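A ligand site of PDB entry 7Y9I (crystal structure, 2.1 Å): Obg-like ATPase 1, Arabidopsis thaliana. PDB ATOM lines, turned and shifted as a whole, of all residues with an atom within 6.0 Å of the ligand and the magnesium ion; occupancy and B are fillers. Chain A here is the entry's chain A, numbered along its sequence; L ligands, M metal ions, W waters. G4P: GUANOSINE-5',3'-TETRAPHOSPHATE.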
ATOM      1  N   GLY A  31     -32.274  -7.895  29.379  1.00  0.00           N
ATOM      2  CA  GLY A  31     -32.976  -6.628  29.122  1.00  0.00           C
ATOM      3  C   GLY A  31     -34.079  -6.823  28.101  1.00  0.00           C
ATOM      4  O   GLY A  31     -34.200  -7.942  27.557  1.00  0.00           O
ATOM      5  N   LEU A  32     -34.856  -5.782  27.820  1.00  0.00           N
ATOM      6  CA  LEU A  32     -35.914  -5.873  26.788  1.00  0.00           C
ATOM      7  C   LEU A  32     -35.252  -6.004  25.423  1.00  0.00           C
ATOM      8  O   LEU A  32     -34.054  -5.778  25.282  1.00  0.00           O
ATOM      9  CB  LEU A  32     -36.839  -4.664  26.919  1.00  0.00           C
ATOM     10  CG  LEU A  32     -37.664  -4.634  28.213  1.00  0.00           C
ATOM     11  CD1 LEU A  32     -38.232  -3.252  28.466  1.00  0.00           C
ATOM     12  CD2 LEU A  32     -38.795  -5.657  28.159  1.00  0.00           C
ATOM     13  N   PRO A  33     -36.013  -6.422  24.379  1.00  0.00           N
ATOM     14  CA  PRO A  33     -35.492  -6.471  23.023  1.00  0.00           C
ATOM     15  C   PRO A  33     -35.024  -5.100  22.527  1.00  0.00           C
ATOM     16  O   PRO A  33     -35.610  -4.100  22.939  1.00  0.00           O
ATOM     17  CB  PRO A  33     -36.688  -6.955  22.169  1.00  0.00           C
ATOM     18  CG  PRO A  33     -37.598  -7.645  23.168  1.00  0.00           C
ATOM     19  CD  PRO A  33     -37.394  -6.916  24.476  1.00  0.00           C
ATOM     20  N   ASN A  34     -34.040  -5.106  21.626  1.00  0.00           N
ATOM     21  CA  ASN A  34     -33.544  -3.922  20.887  1.00  0.00           C
ATOM     22  C   ASN A  34     -32.824  -2.923  21.807  1.00  0.00           C
ATOM     23  O   ASN A  34     -32.805  -1.727  21.455  1.00  0.00           O
ATOM     24  CB  ASN A  34     -34.688  -3.217  20.151  1.00  0.00           C
ATOM     25  CG  ASN A  34     -35.594  -4.209  19.444  1.00  0.00           C
ATOM     26  OD1 ASN A  34     -36.801  -4.214  19.660  1.00  0.00           O
ATOM     27  ND2 ASN A  34     -34.991  -5.053  18.631  1.00  0.00           N
ATOM     28  N   VAL A  35     -32.214  -3.365  22.906  1.00  0.00           N
ATOM     29  CA  VAL A  35     -31.442  -2.447  23.793  1.00  0.00           C
ATOM     30  C   VAL A  35     -29.944  -2.557  23.509  1.00  0.00           C
ATOM     31  O   VAL A  35     -29.215  -1.703  24.010  1.00  0.00           O
ATOM     32  CB  VAL A  35     -31.787  -2.672  25.283  1.00  0.00           C
ATOM     33  CG1 VAL A  35     -33.284  -2.520  25.504  1.00  0.00           C
ATOM     34  CG2 VAL A  35     -31.282  -4.007  25.791  1.00  0.00           C
ATOM     35  N   GLY A  36     -29.501  -3.546  22.719  1.00  0.00           N
ATOM     36  CA  GLY A  36     -28.096  -3.696  22.280  1.00  0.00           C
ATOM     37  C   GLY A  36     -27.364  -4.839  23.003  1.00  0.00           C
ATOM     38  O   GLY A  36     -26.111  -4.791  23.081  1.00  0.00           O
ATOM     39  N   LYS A  37     -28.099  -5.834  23.512  1.00  0.00           N
ATOM     40  CA  LYS A  37     -27.513  -6.995  24.224  1.00  0.00           C
ATOM     41  C   LYS A  37     -26.620  -7.785  23.255  1.00  0.00           C
ATOM     42  O   LYS A  37     -25.412  -7.983  23.570  1.00  0.00           O
ATOM     43  CB  LYS A  37     -28.615  -7.872  24.825  1.00  0.00           C
ATOM     44  CG  LYS A  37     -29.475  -7.190  25.878  1.00  0.00           C
ATOM     45  CD  LYS A  37     -30.375  -8.166  26.620  1.00  0.00           C
ATOM     46  CE  LYS A  37     -31.381  -8.897  25.751  1.00  0.00           C
ATOM     47  NZ  LYS A  37     -32.267  -7.967  24.999  1.00  0.00           N
ATOM     48  N   SER A  38     -27.154  -8.175  22.095  1.00  0.00           N
ATOM     49  CA  SER A  38     -26.428  -9.024  21.118  1.00  0.00           C
ATOM     50  C   SER A  38     -25.285  -8.235  20.479  1.00  0.00           C
ATOM     51  O   SER A  38     -24.224  -8.829  20.205  1.00  0.00           O
ATOM     52  CB  SER A  38     -27.360  -9.639  20.099  1.00  0.00           C
ATOM     53  OG  SER A  38     -28.231 -10.566  20.745  1.00  0.00           O
ATOM     54  N   THR A  39     -25.458  -6.921  20.329  1.00  0.00           N
ATOM     55  CA  THR A  39     -24.382  -6.023  19.835  1.00  0.00           C
ATOM     56  C   THR A  39     -23.254  -5.995  20.865  1.00  0.00           C
ATOM     57  O   THR A  39     -22.087  -6.199  20.468  1.00  0.00           O
ATOM     58  CB  THR A  39     -24.935  -4.625  19.537  1.00  0.00           C
ATOM     59  OG1 THR A  39     -26.065  -4.806  18.675  1.00  0.00           O
ATOM     60  CG2 THR A  39     -23.904  -3.732  18.890  1.00  0.00           C
ATOM     61  N   LEU A  40     -23.579  -5.776  22.140  1.00  0.00           N
ATOM     62  CA  LEU A  40     -22.554  -5.795  23.227  1.00  0.00           C
ATOM     63  C   LEU A  40     -21.842  -7.155  23.221  1.00  0.00           C
ATOM     64  O   LEU A  40     -20.589  -7.169  23.291  1.00  0.00           O
ATOM     65  CB  LEU A  40     -23.225  -5.536  24.565  1.00  0.00           C
ATOM     66  CG  LEU A  40     -22.309  -5.656  25.775  1.00  0.00           C
ATOM     67  CD1 LEU A  40     -21.118  -4.725  25.633  1.00  0.00           C
ATOM     68  CD2 LEU A  40     -23.071  -5.343  27.053  1.00  0.00           C
ATOM     69  N   ASP A  94     -25.088 -14.342  26.151  1.00  0.00           N
ATOM     70  CA  ASP A  94     -26.199 -13.573  25.529  1.00  0.00           C
ATOM     71  C   ASP A  94     -27.508 -14.355  25.687  1.00  0.00           C
ATOM     72  O   ASP A  94     -27.575 -15.476  25.188  1.00  0.00           O
ATOM     73  CB  ASP A  94     -25.900 -13.304  24.052  1.00  0.00           C
ATOM     74  CG  ASP A  94     -26.872 -12.344  23.405  1.00  0.00           C
ATOM     75  OD1 ASP A  94     -27.619 -11.657  24.144  1.00  0.00           O
ATOM     76  OD2 ASP A  94     -26.868 -12.280  22.156  1.00  0.00           O
ATOM     77  N   ILE A  95     -28.495 -13.775  26.374  1.00  0.00           N
ATOM     78  CA  ILE A  95     -29.874 -14.308  26.524  1.00  0.00           C
ATOM     79  C   ILE A  95     -30.787 -13.571  25.535  1.00  0.00           C
ATOM     80  O   ILE A  95     -30.739 -12.324  25.518  1.00  0.00           O
ATOM     81  CB  ILE A  95     -30.357 -14.129  27.984  1.00  0.00           C
ATOM     82  CG1 ILE A  95     -29.283 -14.516  29.003  1.00  0.00           C
ATOM     83  CG2 ILE A  95     -31.659 -14.871  28.209  1.00  0.00           C
ATOM     84  CD1 ILE A  95     -28.749 -15.919  28.853  1.00  0.00           C
ATOM     85  N   ALA A  96     -31.571 -14.316  24.741  1.00  0.00           N
ATOM     86  CA  ALA A  96     -32.374 -13.797  23.594  1.00  0.00           C
ATOM     87  C   ALA A  96     -33.600 -13.013  24.067  1.00  0.00           C
ATOM     88  O   ALA A  96     -33.873 -11.932  23.487  1.00  0.00           O
ATOM     89  CB  ALA A  96     -32.787 -14.945  22.697  1.00  0.00           C
ATOM     90  N   PHE A 129     -30.930   5.578  24.689  1.00  0.00           N
ATOM     91  CA  PHE A 129     -30.555   6.214  23.386  1.00  0.00           C
ATOM     92  C   PHE A 129     -31.833   6.548  22.611  1.00  0.00           C
ATOM     93  O   PHE A 129     -32.789   5.746  22.648  1.00  0.00           O
ATOM     94  CB  PHE A 129     -29.630   5.322  22.577  1.00  0.00           C
ATOM     95  CG  PHE A 129     -30.124   3.926  22.315  1.00  0.00           C
ATOM     96  CD1 PHE A 129     -30.989   3.652  21.267  1.00  0.00           C
ATOM     97  CD2 PHE A 129     -29.689   2.867  23.106  1.00  0.00           C
ATOM     98  CE1 PHE A 129     -31.432   2.361  21.019  1.00  0.00           C
ATOM     99  CE2 PHE A 129     -30.126   1.562  22.865  1.00  0.00           C
ATOM    100  CZ  PHE A 129     -30.994   1.321  21.815  1.00  0.00           C
ATOM    101  N   GLU A 130     -31.810   7.675  21.894  1.00  0.00           N
ATOM    102  CA  GLU A 130     -32.936   8.194  21.074  1.00  0.00           C
ATOM    103  C   GLU A 130     -32.366   8.618  19.713  1.00  0.00           C
ATOM    104  O   GLU A 130     -31.277   9.189  19.704  1.00  0.00           O
ATOM    105  CB  GLU A 130     -33.587   9.415  21.741  1.00  0.00           C
ATOM    106  CG  GLU A 130     -34.312   9.087  23.038  1.00  0.00           C
ATOM    107  N   ASP A 131     -33.119   8.403  18.636  1.00  0.00           N
ATOM    108  CA  ASP A 131     -32.807   8.879  17.268  1.00  0.00           C
ATOM    109  C   ASP A 131     -33.062  10.390  17.168  1.00  0.00           C
ATOM    110  O   ASP A 131     -33.635  10.958  18.119  1.00  0.00           O
ATOM    111  CB  ASP A 131     -33.632   8.115  16.231  1.00  0.00           C
ATOM    112  CG  ASP A 131     -33.501   6.610  16.334  1.00  0.00           C
ATOM    113  OD1 ASP A 131     -32.358   6.134  16.461  1.00  0.00           O
ATOM    114  OD2 ASP A 131     -34.539   5.936  16.282  1.00  0.00           O
ATOM    115  N   ASN A 230     -27.053   2.018  28.089  1.00  0.00           N
ATOM    116  CA  ASN A 230     -26.634   2.165  26.670  1.00  0.00           C
ATOM    117  C   ASN A 230     -27.056   3.557  26.178  1.00  0.00           C
ATOM    118  O   ASN A 230     -28.276   3.839  26.122  1.00  0.00           O
ATOM    119  CB  ASN A 230     -27.223   1.060  25.816  1.00  0.00           C
ATOM    120  CG  ASN A 230     -26.547   0.971  24.477  1.00  0.00           C
ATOM    121  OD1 ASN A 230     -25.646   1.771  24.188  1.00  0.00           O
ATOM    122  ND2 ASN A 230     -26.959   0.026  23.642  1.00  0.00           N
ATOM    123  N   LEU A 231     -26.082   4.363  25.780  1.00  0.00           N
ATOM    124  CA  LEU A 231     -26.233   5.768  25.351  1.00  0.00           C
ATOM    125  C   LEU A 231     -25.753   5.884  23.906  1.00  0.00           C
ATOM    126  O   LEU A 231     -24.853   5.109  23.513  1.00  0.00           O
ATOM    127  CB  LEU A 231     -25.352   6.631  26.260  1.00  0.00           C
ATOM    128  CG  LEU A 231     -25.696   6.610  27.748  1.00  0.00           C
ATOM    129  CD1 LEU A 231     -24.668   7.382  28.549  1.00  0.00           C
ATOM    130  CD2 LEU A 231     -27.070   7.172  27.997  1.00  0.00           C
ATOM    131  N   SER A 263     -21.691   3.346  25.361  1.00  0.00           N
ATOM    132  CA  SER A 263     -22.318   3.446  24.024  1.00  0.00           C
ATOM    133  C   SER A 263     -22.025   2.175  23.217  1.00  0.00           C
ATOM    134  O   SER A 263     -20.867   1.973  22.818  1.00  0.00           O
ATOM    135  CB  SER A 263     -21.848   4.676  23.314  1.00  0.00           C
ATOM    136  OG  SER A 263     -22.433   4.722  22.026  1.00  0.00           O
ATOM    137  N   GLY A 264     -23.039   1.346  22.984  1.00  0.00           N
ATOM    138  CA  GLY A 264     -22.925   0.112  22.175  1.00  0.00           C
ATOM    139  C   GLY A 264     -22.438   0.403  20.774  1.00  0.00           C
ATOM    140  O   GLY A 264     -21.549  -0.317  20.288  1.00  0.00           O
ATOM    141  N   VAL A 265     -22.966   1.464  20.143  1.00  0.00           N
ATOM    142  CA  VAL A 265     -22.584   1.861  18.758  1.00  0.00           C
ATOM    143  C   VAL A 265     -21.100   2.271  18.737  1.00  0.00           C
ATOM    144  O   VAL A 265     -20.406   1.878  17.784  1.00  0.00           O
ATOM    145  CB  VAL A 265     -23.502   2.956  18.189  1.00  0.00           C
ATOM    146  CG1 VAL A 265     -22.984   3.521  16.879  1.00  0.00           C
ATOM    147  CG2 VAL A 265     -24.921   2.431  18.019  1.00  0.00           C
ATOM    148  N   ARG A 268     -18.889  -0.921  19.366  1.00  0.00           N
ATOM    149  CA  ARG A 268     -18.888  -1.755  18.122  1.00  0.00           C
ATOM    150  C   ARG A 268     -17.866  -1.170  17.131  1.00  0.00           C
ATOM    151  O   ARG A 268     -17.013  -1.937  16.611  1.00  0.00           O
ATOM    152  CB  ARG A 268     -20.268  -1.844  17.471  1.00  0.00           C
ATOM    153  CG  ARG A 268     -20.264  -2.558  16.125  1.00  0.00           C
ATOM    154  CD  ARG A 268     -21.642  -2.813  15.553  1.00  0.00           C
ATOM    155  NE  ARG A 268     -22.424  -1.585  15.446  1.00  0.00           N
ATOM    156  CZ  ARG A 268     -23.748  -1.518  15.374  1.00  0.00           C
ATOM    157  NH1 ARG A 268     -24.480  -2.618  15.378  1.00  0.00           N
ATOM    158  NH2 ARG A 268     -24.338  -0.341  15.301  1.00  0.00           N
HETATM  159  PB  G4P L   1     -30.998  -7.044  21.635  1.00  0.00           P
HETATM  160  O1B G4P L   1     -32.443  -7.456  21.396  1.00  0.00           O
HETATM  161  O2B G4P L   1     -30.903  -6.244  22.936  1.00  0.00           O
HETATM  162  O3B G4P L   1     -30.007  -8.193  21.550  1.00  0.00           O
HETATM  163  O3A G4P L   1     -30.537  -5.927  20.575  1.00  0.00           O
HETATM  164  PA  G4P L   1     -29.427  -6.072  19.406  1.00  0.00           P
HETATM  165  O1A G4P L   1     -29.712  -7.421  18.760  1.00  0.00           O
HETATM  166  O2A G4P L   1     -28.054  -5.666  19.850  1.00  0.00           O
HETATM  167  O5' G4P L   1     -29.870  -4.928  18.370  1.00  0.00           O
HETATM  168  C5' G4P L   1     -31.177  -5.079  17.806  1.00  0.00           C
HETATM  169  C4' G4P L   1     -31.687  -3.762  17.258  1.00  0.00           C
HETATM  170  O4' G4P L   1     -31.986  -2.832  18.315  1.00  0.00           O
HETATM  171  C3' G4P L   1     -30.742  -3.077  16.288  1.00  0.00           C
HETATM  172  O3' G4P L   1     -30.928  -3.560  14.941  1.00  0.00           O
HETATM  173  C2' G4P L   1     -31.140  -1.626  16.488  1.00  0.00           C
HETATM  174  O2' G4P L   1     -32.364  -1.260  15.844  1.00  0.00           O
HETATM  175  C1' G4P L   1     -31.487  -1.549  17.940  1.00  0.00           C
HETATM  176  N9  G4P L   1     -30.280  -1.196  18.702  1.00  0.00           N
HETATM  177  C8  G4P L   1     -29.472  -2.022  19.434  1.00  0.00           C
HETATM  178  N7  G4P L   1     -28.473  -1.312  19.992  1.00  0.00           N
HETATM  179  C5  G4P L   1     -28.611  -0.036  19.624  1.00  0.00           C
HETATM  180  C6  G4P L   1     -27.893   1.227  19.871  1.00  0.00           C
HETATM  181  O6  G4P L   1     -26.906   1.197  20.600  1.00  0.00           O
HETATM  182  N1  G4P L   1     -28.364   2.359  19.287  1.00  0.00           N
HETATM  183  C2  G4P L   1     -29.478   2.328  18.507  1.00  0.00           C
HETATM  184  N2  G4P L   1     -29.944   3.453  17.944  1.00  0.00           N
HETATM  185  N3  G4P L   1     -30.185   1.200  18.240  1.00  0.00           N
HETATM  186  C4  G4P L   1     -29.804   0.035  18.769  1.00  0.00           C
HETATM  187  PC  G4P L   1     -29.769  -3.541  13.803  1.00  0.00           P
HETATM  188  O1C G4P L   1     -30.250  -4.287  12.569  1.00  0.00           O
HETATM  189  O2C G4P L   1     -28.458  -4.002  14.376  1.00  0.00           O
HETATM  190  O3C G4P L   1     -29.773  -1.958  13.509  1.00  0.00           O
HETATM  191  PD  G4P L   1     -30.851  -1.270  12.516  1.00  0.00           P
HETATM  192  O1D G4P L   1     -31.139   0.089  13.125  1.00  0.00           O
HETATM  193  O2D G4P L   1     -30.047  -1.298  11.228  1.00  0.00           O
HETATM  194  O3D G4P L   1     -32.097  -2.124  12.485  1.00  0.00           O
HETATM  195 MG    MG M   1     -30.288 -10.308  21.178  1.00  0.00          MG
HETATM  196  O   HOH W   1     -33.516   2.006  17.952  1.00  0.00           O
HETATM  197  O   HOH W   2     -29.819 -10.798  23.065  1.00  0.00           O
HETATM  198  O   HOH W   3     -32.567 -10.090  21.477  1.00  0.00           O
HETATM  199  O   HOH W   4     -30.462  -9.777  19.261  1.00  0.00           O
HETATM  200  O   HOH W   5     -30.733 -12.434  20.782  1.00  0.00           O
HETATM  201  O   HOH W   6     -27.071   4.874  19.869  1.00  0.00           O
HETATM  202  O   HOH W   7     -25.272   3.320  21.246  1.00  0.00           O
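O2A of the ligand is in hydrogen-bond range of OG1 of Thr 39 (2.5 Å).
An oxygen (O2B) of the ligand lies within hydrogen-bond range of the backbone NH of Gly 36 (3.0 Å).
N of Lys 37 is in hydrogen-bond range of O2B of the ligand.
The backbone NH (N) of Asn 34 lies within hydrogen-bond range of an oxygen (O1B) of the ligand (2.9 Å).
N of Thr 39 is in hydrogen-bond range of O2A of the ligand, at 2.9 Å.
O6 of the ligand lies within hydrogen-bond range of ND2 of Asn 230, 3.3 Å away.
NZ of Lys 37 is in salt-bridge range of O2B of the ligand, at 3.0 Å.
O2A of the ligand is in hydrogen-bond range of N of Ser 38 (3.5 Å).
N of Val 35 is in hydrogen-bond range of O2B of the ligand, 3.2 Å away.
Of the 22 residues printed, 1 comes within 4 Å of the magnesium ion.
The nearest printed residue that does not touch the magnesium ion is Asp 94 (4.1 Å).
Water W2 lies within hydrogen-bond range of OD1 of Asp 94 (2.6 Å) and O of Ile 95 (3.0 Å).
Water W3 bridges an oxygen (O1B) of the ligand (2.6 Å) and the backbone carbonyl oxygen of Ala 96 (3.0 Å).
Leu 32 touches the ligand.
Pro 33 touches the ligand (CA to O1B, 3.6 Å).
CE1 of Phe 129 touches C2 of the ligand, at 3.2 Å.
OD1 of Asp 131 touches N2 of the ligand, at 3.9 Å.
Val 265 touches the ligand.
Within 4 Å of the ligand: Leu 32, Pro 33, Asn 34, Val 35, Gly 36, Lys 37, Ser 38, Thr 39, Phe 129, Asp 131, Asn 230 and Val 265.
The magnesium ion is bound by water W4, water W2, the side-chain hydroxyl of Ser 38, an oxygen (O3B) of the ligand, water W5 and water W3.
The magnesium ion has six donor atoms within binding distance.
NZ of Lys 37 sits at hydrogen-bond distance from O of Leu 32, at 2.8 Å.
The side-chain carboxylate of Asp 94 lies close to the side-chain hydroxyl of Ser 38 (2.6 Å).
N of Phe 129 lies close to O of Asn 230 (3.5 Å).
The backbone NH (N) of Gly 264 sits at hydrogen-bond distance from the side-chain amide oxygen (OD1) of Asn 230, 2.9 Å away.
The side-chain amino group (NZ) of Lys 37 sits at hydrogen-bond distance from the backbone carbonyl oxygen (O) of Gly 31 (3.2 Å).
ND2 of Asn 230 lies within hydrogen-bond range of O of Val 35 (2.9 Å).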
